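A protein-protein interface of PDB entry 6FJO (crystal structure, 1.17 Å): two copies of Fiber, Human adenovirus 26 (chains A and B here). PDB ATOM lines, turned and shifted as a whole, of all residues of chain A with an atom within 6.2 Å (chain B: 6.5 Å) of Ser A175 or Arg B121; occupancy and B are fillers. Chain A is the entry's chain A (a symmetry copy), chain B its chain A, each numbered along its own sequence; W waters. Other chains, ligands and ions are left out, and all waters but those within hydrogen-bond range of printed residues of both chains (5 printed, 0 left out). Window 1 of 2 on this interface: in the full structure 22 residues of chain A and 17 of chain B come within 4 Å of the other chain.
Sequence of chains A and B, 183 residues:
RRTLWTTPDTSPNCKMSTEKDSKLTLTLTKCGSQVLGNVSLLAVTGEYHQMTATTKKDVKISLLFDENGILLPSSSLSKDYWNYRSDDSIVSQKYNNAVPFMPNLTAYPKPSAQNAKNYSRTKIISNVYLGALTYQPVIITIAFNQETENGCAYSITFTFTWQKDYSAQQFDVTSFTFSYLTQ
O of Arg B121 sits at hydrogen-bond distance from OG of Ser A175 (2.7 Å).
The side-chain hydroxyl (OG1) of Thr A177 lies within hydrogen-bond range of the side-chain hydroxyl (OG) of Ser B179 (2.8 Å).
The backbone carbonyl oxygen of Pro A8 lies close to the backbone carbonyl oxygen of Thr B106 (3.3 Å).
NH2 of Arg B121 lies within hydrogen-bond range of O of Pro A8 (2.8 Å).
O of Asp A9 sits at hydrogen-bond distance from NH1 of Arg B121 (3.0 Å).
The backbone carbonyl oxygen of Ser B179 lies within hydrogen-bond range of the side-chain amide nitrogen of Asn A38 (3.5 Å).
The backbone NH (N) of Ser B120 is in hydrogen-bond range of the side-chain carboxylate (OD2) of Asp A172 (2.8 Å).
The guanidinium group (NH1) of Arg B121 sits at hydrogen-bond distance from the side-chain hydroxyl (OG1) of Thr A25 (2.8 Å).
The side-chain hydroxyl (OG1) of Thr A10 sits at hydrogen-bond distance from the side-chain hydroxyl (OH) of Tyr B119, 3.4 Å away.
O of Lys B123 sits at hydrogen-bond distance from N of Ser A175 (2.9 Å).
The side-chain carboxylate of Asp A9 lies within hydrogen-bond range of the side-chain hydroxyl of Thr A7 (3.4 Å).
N of Val A173 lies within hydrogen-bond range of O of Leu A41 (3.2 Å).
The backbone carbonyl oxygen (O) of Tyr B119 lies within hydrogen-bond range of the side-chain hydroxyl (OG1) of Thr B122, 2.8 Å away.
O of Ser A40 sits at hydrogen-bond distance from N of Thr A25 (2.8 Å).
The side-chain hydroxyl (OG1) of Thr A177 sits at hydrogen-bond distance from the side-chain amide nitrogen (ND2) of Asn A38, 3.4 Å away.
The backbone carbonyl oxygen (O) of Ala B107 sits at hydrogen-bond distance from the guanidinium group (NE) of Arg B121.
N of Ala B107 touches CB of Pro A8, 3.6 Å away.
CG2 of Thr A10 touches NH2 of Arg B121, at 3.5 Å.
Ser A40 touches Arg B121.
C of Tyr B119 touches OD2 of Asp A172 (3.7 Å).
Val A173 touches Ser B120.
O of Val A173 touches N of Arg B121 (3.6 Å).
Thr A174 touches Ser B120.
Lys B123 touches Thr A174 (O to CB, 3.2 Å).
Thr A174 touches Ile B125.
CG1 of Ile B124 touches O of Ser A175 (3.8 Å).
Of chain B, only Arg B121 (2.7 Å), Lys B123 (2.9 Å) and Ile B124 (3.8 Å) come within 4 Å of Ser A175.
Of the printed residues of chain A, Arg B121 touches Pro A8, Asp A9, Thr A10, Thr A25, Ser A40, Val A173 and Ser A175.
Of the printed residues of chain A, Ser B120 touches Asp A172, Val A173 and Thr A174.
Of the printed residues of chain A, Lys B123 touches Thr A174 (3.2 Å) and Ser A175 (2.9 Å).
Of the printed residues of chain A, Ser B179 touches Asn A38 (3.5 Å) and Thr A177 (2.8 Å).
Of the printed residues of chain B, Asp A9 touches Arg B121.
Printed residues of chain B within 4 Å of Thr A25: Arg B121 (2.8 Å).
Thr B122 touches none of the printed residues of chain A.
Val A39 touches none of the printed residues of chain B.
The nearest printed residue of chain A that does not touch Ser B179 is Ser A175 (5.9 Å).
Of the 14 printed residues of chain B, 9 touch a printed residue of chain A.
Hydrophobic or aromatic side chains of chain B within 4 Å of the printed part of chain A: Ala B107, Tyr B119, Ile B124 and Ile B125.
Of the 17 printed residues of chain A, 11 touch a printed residue of chain B.
Among the printed residues, no Asp or Glu carboxylate lies within 4 Å of a Lys or Arg side-chain nitrogen of the other chain.
No position is printed for both chains.
Of the 20 pairs that touch across the chains among the printed residues, none has its exchanged pair printed and touching as well.
Water W3 bridges the backbone carbonyl oxygen of Arg B121 (2.6 Å) and the side-chain hydroxyl of Ser A175 (3.3 Å).
Water W4 lies within hydrogen-bond range of the side-chain amide oxygen of Asn A38 (2.7 Å), the side-chain hydroxyl of Tyr B108 (2.7 Å) and the side-chain hydroxyl of Ser A175 (2.9 Å).
Water W2 lies within hydrogen-bond range of OG1 of Thr A174 (2.7 Å), O of Ser A175 (2.7 Å) and N of Ile B125 (3.0 Å).
Water W1 lies within hydrogen-bond range of the backbone carbonyl oxygen (O) of Ser B179 (2.7 Å) and the side-chain amide nitrogen (ND2) of Asn A38 (2.9 Å).
Water W5 lies within hydrogen-bond range of OD1 of Asp A172, N of Arg B121 and N of Ser B120.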
ATOM      1  N   THR A   7      15.581  27.349   6.560  1.00  0.00           N
ATOM      2  CA  THR A   7      16.162  28.418   5.777  1.00  0.00           C
ATOM      3  C   THR A   7      17.487  28.800   6.423  1.00  0.00           C
ATOM      4  O   THR A   7      17.732  28.607   7.648  1.00  0.00           O
ATOM      5  CB  THR A   7      15.255  29.675   5.582  1.00  0.00           C
ATOM      6  OG1 THR A   7      15.288  30.498   6.753  1.00  0.00           O
ATOM      7  CG2 THR A   7      13.806  29.193   5.352  1.00  0.00           C
ATOM      8  N   PRO A   8      18.337  29.387   5.585  1.00  0.00           N
ATOM      9  CA  PRO A   8      19.666  29.779   6.103  1.00  0.00           C
ATOM     10  C   PRO A   8      19.793  31.229   6.593  1.00  0.00           C
ATOM     11  O   PRO A   8      20.906  31.733   6.691  1.00  0.00           O
ATOM     12  CB  PRO A   8      20.533  29.578   4.864  1.00  0.00           C
ATOM     13  CG  PRO A   8      19.677  29.880   3.728  1.00  0.00           C
ATOM     14  CD  PRO A   8      18.348  29.277   4.118  1.00  0.00           C
ATOM     15  N   ASP A   9      18.701  31.939   6.842  1.00  0.00           N
ATOM     16  CA  ASP A   9      18.770  33.336   7.270  1.00  0.00           C
ATOM     17  C   ASP A   9      19.047  33.358   8.793  1.00  0.00           C
ATOM     18  O   ASP A   9      19.404  32.313   9.374  1.00  0.00           O
ATOM     19  CB  ASP A   9      17.493  34.074   6.836  1.00  0.00           C
ATOM     20  CG  ASP A   9      16.245  33.691   7.637  1.00  0.00           C
ATOM     21  OD1 ASP A   9      16.325  33.054   8.709  1.00  0.00           O
ATOM     22  OD2 ASP A   9      15.154  34.061   7.185  1.00  0.00           O
ATOM     23  N   THR A  10      18.976  34.538   9.428  1.00  0.00           N
ATOM     24  CA  THR A  10      19.199  34.600  10.869  1.00  0.00           C
ATOM     25  C   THR A  10      17.968  35.106  11.640  1.00  0.00           C
ATOM     26  O   THR A  10      18.070  35.578  12.802  1.00  0.00           O
ATOM     27  CB  THR A  10      20.446  35.454  11.168  1.00  0.00           C
ATOM     28  OG1 THR A  10      20.334  36.733  10.534  1.00  0.00           O
ATOM     29  CG2 THR A  10      21.705  34.737  10.656  1.00  0.00           C
ATOM     30  N   LYS A  23      18.257  31.582  16.705  1.00  0.00           N
ATOM     31  CA  LYS A  23      18.164  31.021  15.375  1.00  0.00           C
ATOM     32  C   LYS A  23      18.758  29.659  15.377  1.00  0.00           C
ATOM     33  O   LYS A  23      20.004  29.512  15.563  1.00  0.00           O
ATOM     34  CB  LYS A  23      18.865  31.905  14.278  1.00  0.00           C
ATOM     35  CG  LYS A  23      18.990  31.158  12.860  1.00  0.00           C
ATOM     36  CD  LYS A  23      17.723  31.096  11.991  1.00  0.00           C
ATOM     37  CE  LYS A  23      17.848  30.111  10.807  1.00  0.00           C
ATOM     38  NZ  LYS A  23      16.903  30.460   9.738  1.00  0.00           N
ATOM     39  N   THR A  25      19.772  26.906  12.878  1.00  0.00           N
ATOM     40  CA  THR A  25      19.955  26.669  11.467  1.00  0.00           C
ATOM     41  C   THR A  25      20.034  25.146  11.305  1.00  0.00           C
ATOM     42  O   THR A  25      20.931  24.512  11.849  1.00  0.00           O
ATOM     43  CB  THR A  25      21.222  27.336  10.886  1.00  0.00           C
ATOM     44  OG1 THR A  25      21.200  28.705  11.207  1.00  0.00           O
ATOM     45  CG2 THR A  25      21.308  27.147   9.394  1.00  0.00           C
ATOM     46  N   ASN A  38      22.705  18.971   9.105  1.00  0.00           N
ATOM     47  CA  ASN A  38      23.701  20.030   9.380  1.00  0.00           C
ATOM     48  C   ASN A  38      23.020  21.009  10.321  1.00  0.00           C
ATOM     49  O   ASN A  38      21.895  21.479   9.983  1.00  0.00           O
ATOM     50  CB  ASN A  38      24.077  20.628   8.066  1.00  0.00           C
ATOM     51  CG  ASN A  38      25.026  21.689   8.178  1.00  0.00           C
ATOM     52  OD1 ASN A  38      24.655  22.836   8.487  1.00  0.00           O
ATOM     53  ND2 ASN A  38      26.267  21.391   7.957  1.00  0.00           N
ATOM     54  N   VAL A  39      23.609  21.292  11.451  1.00  0.00           N
ATOM     55  CA  VAL A  39      22.944  22.093  12.470  1.00  0.00           C
ATOM     56  C   VAL A  39      23.874  23.108  13.089  1.00  0.00           C
ATOM     57  O   VAL A  39      25.087  22.789  13.319  1.00  0.00           O
ATOM     58  CB  VAL A  39      22.314  21.190  13.551  1.00  0.00           C
ATOM     59  CG1 VAL A  39      23.309  20.384  14.335  1.00  0.00           C
ATOM     60  CG2 VAL A  39      21.371  21.957  14.492  1.00  0.00           C
ATOM     61  N   SER A  40      23.318  24.174  13.620  1.00  0.00           N
ATOM     62  CA  SER A  40      24.023  25.165  14.449  1.00  0.00           C
ATOM     63  C   SER A  40      22.953  26.024  15.074  1.00  0.00           C
ATOM     64  O   SER A  40      21.755  26.014  14.635  1.00  0.00           O
ATOM     65  CB  SER A  40      24.908  26.034  13.568  1.00  0.00           C
ATOM     66  OG  SER A  40      24.162  26.928  12.710  1.00  0.00           O
ATOM     67  N   LEU A  41      23.379  26.748  16.116  1.00  0.00           N
ATOM     68  CA  LEU A  41      22.451  27.507  16.966  1.00  0.00           C
ATOM     69  C   LEU A  41      23.121  28.790  17.393  1.00  0.00           C
ATOM     70  O   LEU A  41      24.312  28.778  17.802  1.00  0.00           O
ATOM     71  CB  LEU A  41      22.101  26.629  18.190  1.00  0.00           C
ATOM     72  CG  LEU A  41      21.155  27.256  19.215  1.00  0.00           C
ATOM     73  CD1 LEU A  41      19.773  27.589  18.640  1.00  0.00           C
ATOM     74  CD2 LEU A  41      21.037  26.335  20.393  1.00  0.00           C
ATOM     75  N   VAL A 128      31.189  20.809  19.424  1.00  0.00           N
ATOM     76  CA  VAL A 128      31.215  21.994  18.584  1.00  0.00           C
ATOM     77  C   VAL A 128      31.899  23.094  19.405  1.00  0.00           C
ATOM     78  O   VAL A 128      32.340  22.825  20.532  1.00  0.00           O
ATOM     79  CB  VAL A 128      29.821  22.398  18.108  1.00  0.00           C
ATOM     80  CG1 VAL A 128      29.242  21.352  17.186  1.00  0.00           C
ATOM     81  CG2 VAL A 128      28.844  22.683  19.280  1.00  0.00           C
ATOM     82  N   ASP A 172      26.876  30.960  20.445  1.00  0.00           N
ATOM     83  CA  ASP A 172      26.915  30.779  18.992  1.00  0.00           C
ATOM     84  C   ASP A 172      27.882  29.656  18.747  1.00  0.00           C
ATOM     85  O   ASP A 172      28.954  29.656  19.421  1.00  0.00           O
ATOM     86  CB  ASP A 172      27.400  32.026  18.283  1.00  0.00           C
ATOM     87  CG  ASP A 172      27.204  31.930  16.740  1.00  0.00           C
ATOM     88  OD1 ASP A 172      26.493  31.064  16.289  1.00  0.00           O
ATOM     89  OD2 ASP A 172      27.727  32.829  16.060  1.00  0.00           O
ATOM     90  N   VAL A 173      27.549  28.661  17.992  1.00  0.00           N
ATOM     91  CA  VAL A 173      28.418  27.510  17.815  1.00  0.00           C
ATOM     92  C   VAL A 173      28.685  27.231  16.341  1.00  0.00           C
ATOM     93  O   VAL A 173      27.920  27.591  15.440  1.00  0.00           O
ATOM     94  CB  VAL A 173      27.870  26.253  18.501  1.00  0.00           C
ATOM     95  CG1 VAL A 173      27.959  26.381  20.033  1.00  0.00           C
ATOM     96  CG2 VAL A 173      26.470  25.874  18.024  1.00  0.00           C
ATOM     97  N   THR A 174      29.813  26.565  16.107  1.00  0.00           N
ATOM     98  CA  THR A 174      30.150  26.055  14.778  1.00  0.00           C
ATOM     99  C   THR A 174      29.129  25.033  14.308  1.00  0.00           C
ATOM    100  O   THR A 174      28.338  24.492  15.092  1.00  0.00           O
ATOM    101  CB  THR A 174      31.563  25.453  14.844  1.00  0.00           C
ATOM    102  OG1 THR A 174      31.660  24.467  15.891  1.00  0.00           O
ATOM    103  CG2 THR A 174      32.614  26.499  15.061  1.00  0.00           C
ATOM    104  N   SER A 175      29.111  24.818  12.995  1.00  0.00           N
ATOM    105  CA  SER A 175      28.177  23.870  12.361  1.00  0.00           C
ATOM    106  C   SER A 175      28.602  22.443  12.599  1.00  0.00           C
ATOM    107  O   SER A 175      29.814  22.099  12.626  1.00  0.00           O
ATOM    108  CB  SER A 175      28.106  24.112  10.878  1.00  0.00           C
ATOM    109  OG  SER A 175      27.455  25.393  10.642  1.00  0.00           O
ATOM    110  N   PHE A 176      27.608  21.553  12.692  1.00  0.00           N
ATOM    111  CA  PHE A 176      27.877  20.137  12.918  1.00  0.00           C
ATOM    112  C   PHE A 176      27.138  19.299  11.889  1.00  0.00           C
ATOM    113  O   PHE A 176      25.894  19.450  11.740  1.00  0.00           O
ATOM    114  CB  PHE A 176      27.442  19.753  14.339  1.00  0.00           C
ATOM    115  CG  PHE A 176      27.780  18.352  14.712  1.00  0.00           C
ATOM    116  CD1 PHE A 176      29.084  17.986  14.881  1.00  0.00           C
ATOM    117  CD2 PHE A 176      26.831  17.361  14.840  1.00  0.00           C
ATOM    118  CE1 PHE A 176      29.405  16.682  15.231  1.00  0.00           C
ATOM    119  CE2 PHE A 176      27.151  16.066  15.162  1.00  0.00           C
ATOM    120  CZ  PHE A 176      28.431  15.738  15.360  1.00  0.00           C
ATOM    121  N   THR A 177      27.812  18.384  11.278  1.00  0.00           N
ATOM    122  CA  THR A 177      27.275  17.442  10.291  1.00  0.00           C
ATOM    123  C   THR A 177      27.009  16.106  10.918  1.00  0.00           C
ATOM    124  O   THR A 177      27.854  15.634  11.722  1.00  0.00           O
ATOM    125  CB  THR A 177      28.227  17.286   9.119  1.00  0.00           C
ATOM    126  OG1 THR A 177      28.206  18.585   8.416  1.00  0.00           O
ATOM    127  CG2 THR A 177      27.844  16.248   8.129  1.00  0.00           C
ATOM    128  N   THR B 106      23.901  32.937   1.845  1.00  0.00           N
ATOM    129  CA  THR B 106      23.017  33.354   2.930  1.00  0.00           C
ATOM    130  C   THR B 106      23.381  32.656   4.226  1.00  0.00           C
ATOM    131  O   THR B 106      23.491  33.263   5.306  1.00  0.00           O
ATOM    132  CB  THR B 106      21.550  33.138   2.569  1.00  0.00           C
ATOM    133  OG1 THR B 106      21.276  33.879   1.376  1.00  0.00           O
ATOM    134  CG2 THR B 106      20.605  33.626   3.689  1.00  0.00           C
ATOM    135  N   ALA B 107      23.632  31.358   4.163  1.00  0.00           N
ATOM    136  CA  ALA B 107      24.091  30.623   5.311  1.00  0.00           C
ATOM    137  C   ALA B 107      25.471  31.113   5.760  1.00  0.00           C
ATOM    138  O   ALA B 107      25.775  31.205   6.984  1.00  0.00           O
ATOM    139  CB  ALA B 107      24.210  29.182   4.979  1.00  0.00           C
ATOM    140  N   TYR B 108      26.320  31.404   4.758  1.00  0.00           N
ATOM    141  CA  TYR B 108      27.735  31.678   5.040  1.00  0.00           C
ATOM    142  C   TYR B 108      28.091  32.971   4.340  1.00  0.00           C
ATOM    143  O   TYR B 108      28.710  32.971   3.251  1.00  0.00           O
ATOM    144  CB  TYR B 108      28.619  30.534   4.570  1.00  0.00           C
ATOM    145  CG  TYR B 108      28.124  29.150   4.887  1.00  0.00           C
ATOM    146  CD1 TYR B 108      27.909  28.732   6.183  1.00  0.00           C
ATOM    147  CD2 TYR B 108      27.844  28.253   3.884  1.00  0.00           C
ATOM    148  CE1 TYR B 108      27.452  27.462   6.461  1.00  0.00           C
ATOM    149  CE2 TYR B 108      27.378  26.989   4.130  1.00  0.00           C
ATOM    150  CZ  TYR B 108      27.180  26.574   5.445  1.00  0.00           C
ATOM    151  OH  TYR B 108      26.725  25.300   5.660  1.00  0.00           O
ATOM    152  N   PRO B 109      27.677  34.129   4.871  1.00  0.00           N
ATOM    153  CA  PRO B 109      27.914  35.368   4.211  1.00  0.00           C
ATOM    154  C   PRO B 109      29.373  35.797   4.332  1.00  0.00           C
ATOM    155  O   PRO B 109      30.071  35.457   5.287  1.00  0.00           O
ATOM    156  CB  PRO B 109      27.012  36.338   4.980  1.00  0.00           C
ATOM    157  CG  PRO B 109      26.913  35.755   6.284  1.00  0.00           C
ATOM    158  CD  PRO B 109      26.865  34.318   6.113  1.00  0.00           C
ATOM    159  N   ASN B 118      31.454  37.371  12.561  1.00  0.00           N
ATOM    160  CA  ASN B 118      30.560  36.672  11.706  1.00  0.00           C
ATOM    161  C   ASN B 118      30.018  35.503  12.534  1.00  0.00           C
ATOM    162  O   ASN B 118      30.479  35.176  13.620  1.00  0.00           O
ATOM    163  CB  ASN B 118      31.214  36.136  10.410  1.00  0.00           C
ATOM    164  CG  ASN B 118      30.262  36.182   9.213  1.00  0.00           C
ATOM    165  OD1 ASN B 118      30.682  36.019   8.026  1.00  0.00           O
ATOM    166  ND2 ASN B 118      29.009  36.403   9.464  1.00  0.00           N
ATOM    167  N   TYR B 119      28.989  34.959  11.969  1.00  0.00           N
ATOM    168  CA  TYR B 119      28.315  33.819  12.534  1.00  0.00           C
ATOM    169  C   TYR B 119      29.246  32.635  12.683  1.00  0.00           C
ATOM    170  O   TYR B 119      29.945  32.301  11.726  1.00  0.00           O
ATOM    171  CB  TYR B 119      27.163  33.536  11.561  1.00  0.00           C
ATOM    172  CG  TYR B 119      26.177  34.676  11.438  1.00  0.00           C
ATOM    173  CD1 TYR B 119      25.557  35.184  12.559  1.00  0.00           C
ATOM    174  CD2 TYR B 119      25.907  35.293  10.189  1.00  0.00           C
ATOM    175  CE1 TYR B 119      24.644  36.227  12.477  1.00  0.00           C
ATOM    176  CE2 TYR B 119      25.024  36.367  10.091  1.00  0.00           C
ATOM    177  CZ  TYR B 119      24.394  36.803  11.245  1.00  0.00           C
ATOM    178  OH  TYR B 119      23.503  37.847  11.173  1.00  0.00           O
ATOM    179  N   SER B 120      29.248  31.981  13.834  1.00  0.00           N
ATOM    180  CA  SER B 120      30.069  30.811  14.001  1.00  0.00           C
ATOM    181  C   SER B 120      29.712  29.660  13.053  1.00  0.00           C
ATOM    182  O   SER B 120      30.525  28.800  12.825  1.00  0.00           O
ATOM    183  CB  SER B 120      30.050  30.330  15.444  1.00  0.00           C
ATOM    184  OG  SER B 120      30.513  31.362  16.322  1.00  0.00           O
ATOM    185  N   ARG B 121      28.460  29.677  12.566  1.00  0.00           N
ATOM    186  CA  ARG B 121      28.056  28.583  11.659  1.00  0.00           C
ATOM    187  C   ARG B 121      28.825  28.553  10.399  1.00  0.00           C
ATOM    188  O   ARG B 121      28.801  27.563   9.655  1.00  0.00           O
ATOM    189  CB  ARG B 121      26.579  28.635  11.374  1.00  0.00           C
ATOM    190  CG  ARG B 121      26.160  29.775  10.495  1.00  0.00           C
ATOM    191  CD  ARG B 121      24.648  29.798  10.280  1.00  0.00           C
ATOM    192  NE  ARG B 121      24.317  30.865   9.325  1.00  0.00           N
ATOM    193  CZ  ARG B 121      23.158  31.450   9.173  1.00  0.00           C
ATOM    194  NH1 ARG B 121      22.018  30.965   9.753  1.00  0.00           N
ATOM    195  NH2 ARG B 121      23.035  32.445   8.306  1.00  0.00           N
ATOM    196  N   THR B 122      29.565  29.621  10.052  1.00  0.00           N
ATOM    197  CA  THR B 122      30.452  29.658   8.896  1.00  0.00           C
ATOM    198  C   THR B 122      31.641  28.777   9.040  1.00  0.00           C
ATOM    199  O   THR B 122      32.408  28.653   8.055  1.00  0.00           O
ATOM    200  CB  THR B 122      30.914  31.117   8.592  1.00  0.00           C
ATOM    201  OG1 THR B 122      31.713  31.595   9.656  1.00  0.00           O
ATOM    202  CG2 THR B 122      29.760  32.031   8.287  1.00  0.00           C
ATOM    203  N   LYS B 123      31.867  28.172  10.215  1.00  0.00           N
ATOM    204  CA  LYS B 123      32.981  27.309  10.419  1.00  0.00           C
ATOM    205  C   LYS B 123      32.537  25.937  10.949  1.00  0.00           C
ATOM    206  O   LYS B 123      31.490  25.819  11.629  1.00  0.00           O
ATOM    207  CB  LYS B 123      33.968  27.895  11.409  1.00  0.00           C
ATOM    208  CG  LYS B 123      34.733  29.058  10.753  1.00  0.00           C
ATOM    209  CD  LYS B 123      35.602  29.775  11.745  1.00  0.00           C
ATOM    210  CE  LYS B 123      36.529  30.809  11.067  1.00  0.00           C
ATOM    211  NZ  LYS B 123      37.308  31.559  12.089  1.00  0.00           N
ATOM    212  N   ILE B 124      33.352  24.964  10.690  1.00  0.00           N
ATOM    213  CA  ILE B 124      33.309  23.618  11.299  1.00  0.00           C
ATOM    214  C   ILE B 124      34.624  23.464  12.003  1.00  0.00           C
ATOM    215  O   ILE B 124      35.698  23.689  11.345  1.00  0.00           O
ATOM    216  CB  ILE B 124      33.137  22.510  10.257  1.00  0.00           C
ATOM    217  CG1 ILE B 124      31.841  22.658   9.508  1.00  0.00           C
ATOM    218  CG2 ILE B 124      33.254  21.119  10.893  1.00  0.00           C
ATOM    219  CD1 ILE B 124      31.870  21.816   8.211  1.00  0.00           C
ATOM    220  N   ILE B 125      34.650  23.042  13.249  1.00  0.00           N
ATOM    221  CA  ILE B 125      35.910  22.809  13.973  1.00  0.00           C
ATOM    222  C   ILE B 125      35.836  21.410  14.573  1.00  0.00           C
ATOM    223  O   ILE B 125      34.858  21.095  15.284  1.00  0.00           O
ATOM    224  CB  ILE B 125      36.156  23.861  15.025  1.00  0.00           C
ATOM    225  CG1 ILE B 125      36.358  25.254  14.400  1.00  0.00           C
ATOM    226  CG2 ILE B 125      37.359  23.506  15.882  1.00  0.00           C
ATOM    227  CD1 ILE B 125      36.493  26.398  15.323  1.00  0.00           C
ATOM    228  N   PHE B 144      33.758  28.731   5.466  1.00  0.00           N
ATOM    229  CA  PHE B 144      33.028  28.952   4.240  1.00  0.00           C
ATOM    230  C   PHE B 144      32.793  30.407   3.978  1.00  0.00           C
ATOM    231  O   PHE B 144      32.214  31.123   4.802  1.00  0.00           O
ATOM    232  CB  PHE B 144      31.675  28.222   4.273  1.00  0.00           C
ATOM    233  CG  PHE B 144      31.836  26.771   4.504  1.00  0.00           C
ATOM    234  CD1 PHE B 144      32.344  25.934   3.534  1.00  0.00           C
ATOM    235  CD2 PHE B 144      31.484  26.203   5.710  1.00  0.00           C
ATOM    236  CE1 PHE B 144      32.538  24.610   3.750  1.00  0.00           C
ATOM    237  CE2 PHE B 144      31.629  24.805   5.936  1.00  0.00           C
ATOM    238  CZ  PHE B 144      32.249  24.073   4.924  1.00  0.00           C
ATOM    239  N   SER B 179      29.882  18.474   5.814  1.00  0.00           N
ATOM    240  CA  SER B 179      28.951  18.890   4.799  1.00  0.00           C
ATOM    241  C   SER B 179      28.724  20.400   4.905  1.00  0.00           C
ATOM    242  O   SER B 179      29.072  21.012   5.961  1.00  0.00           O
ATOM    243  CB  SER B 179      27.635  18.159   4.846  1.00  0.00           C
ATOM    244  OG  SER B 179      26.817  18.601   5.940  1.00  0.00           O
HETATM  245  O   HOH W   1      28.671  23.001   7.792  1.00  0.00           O
HETATM  246  O   HOH W   2      31.891  22.325  14.309  1.00  0.00           O
HETATM  247  O   HOH W   3      29.788  25.531   8.275  1.00  0.00           O
HETATM  248  O   HOH W   4      25.914  25.175   8.253  1.00  0.00           O
HETATM  249  O   HOH W   5      26.268  31.455  13.445  1.00  0.00           O
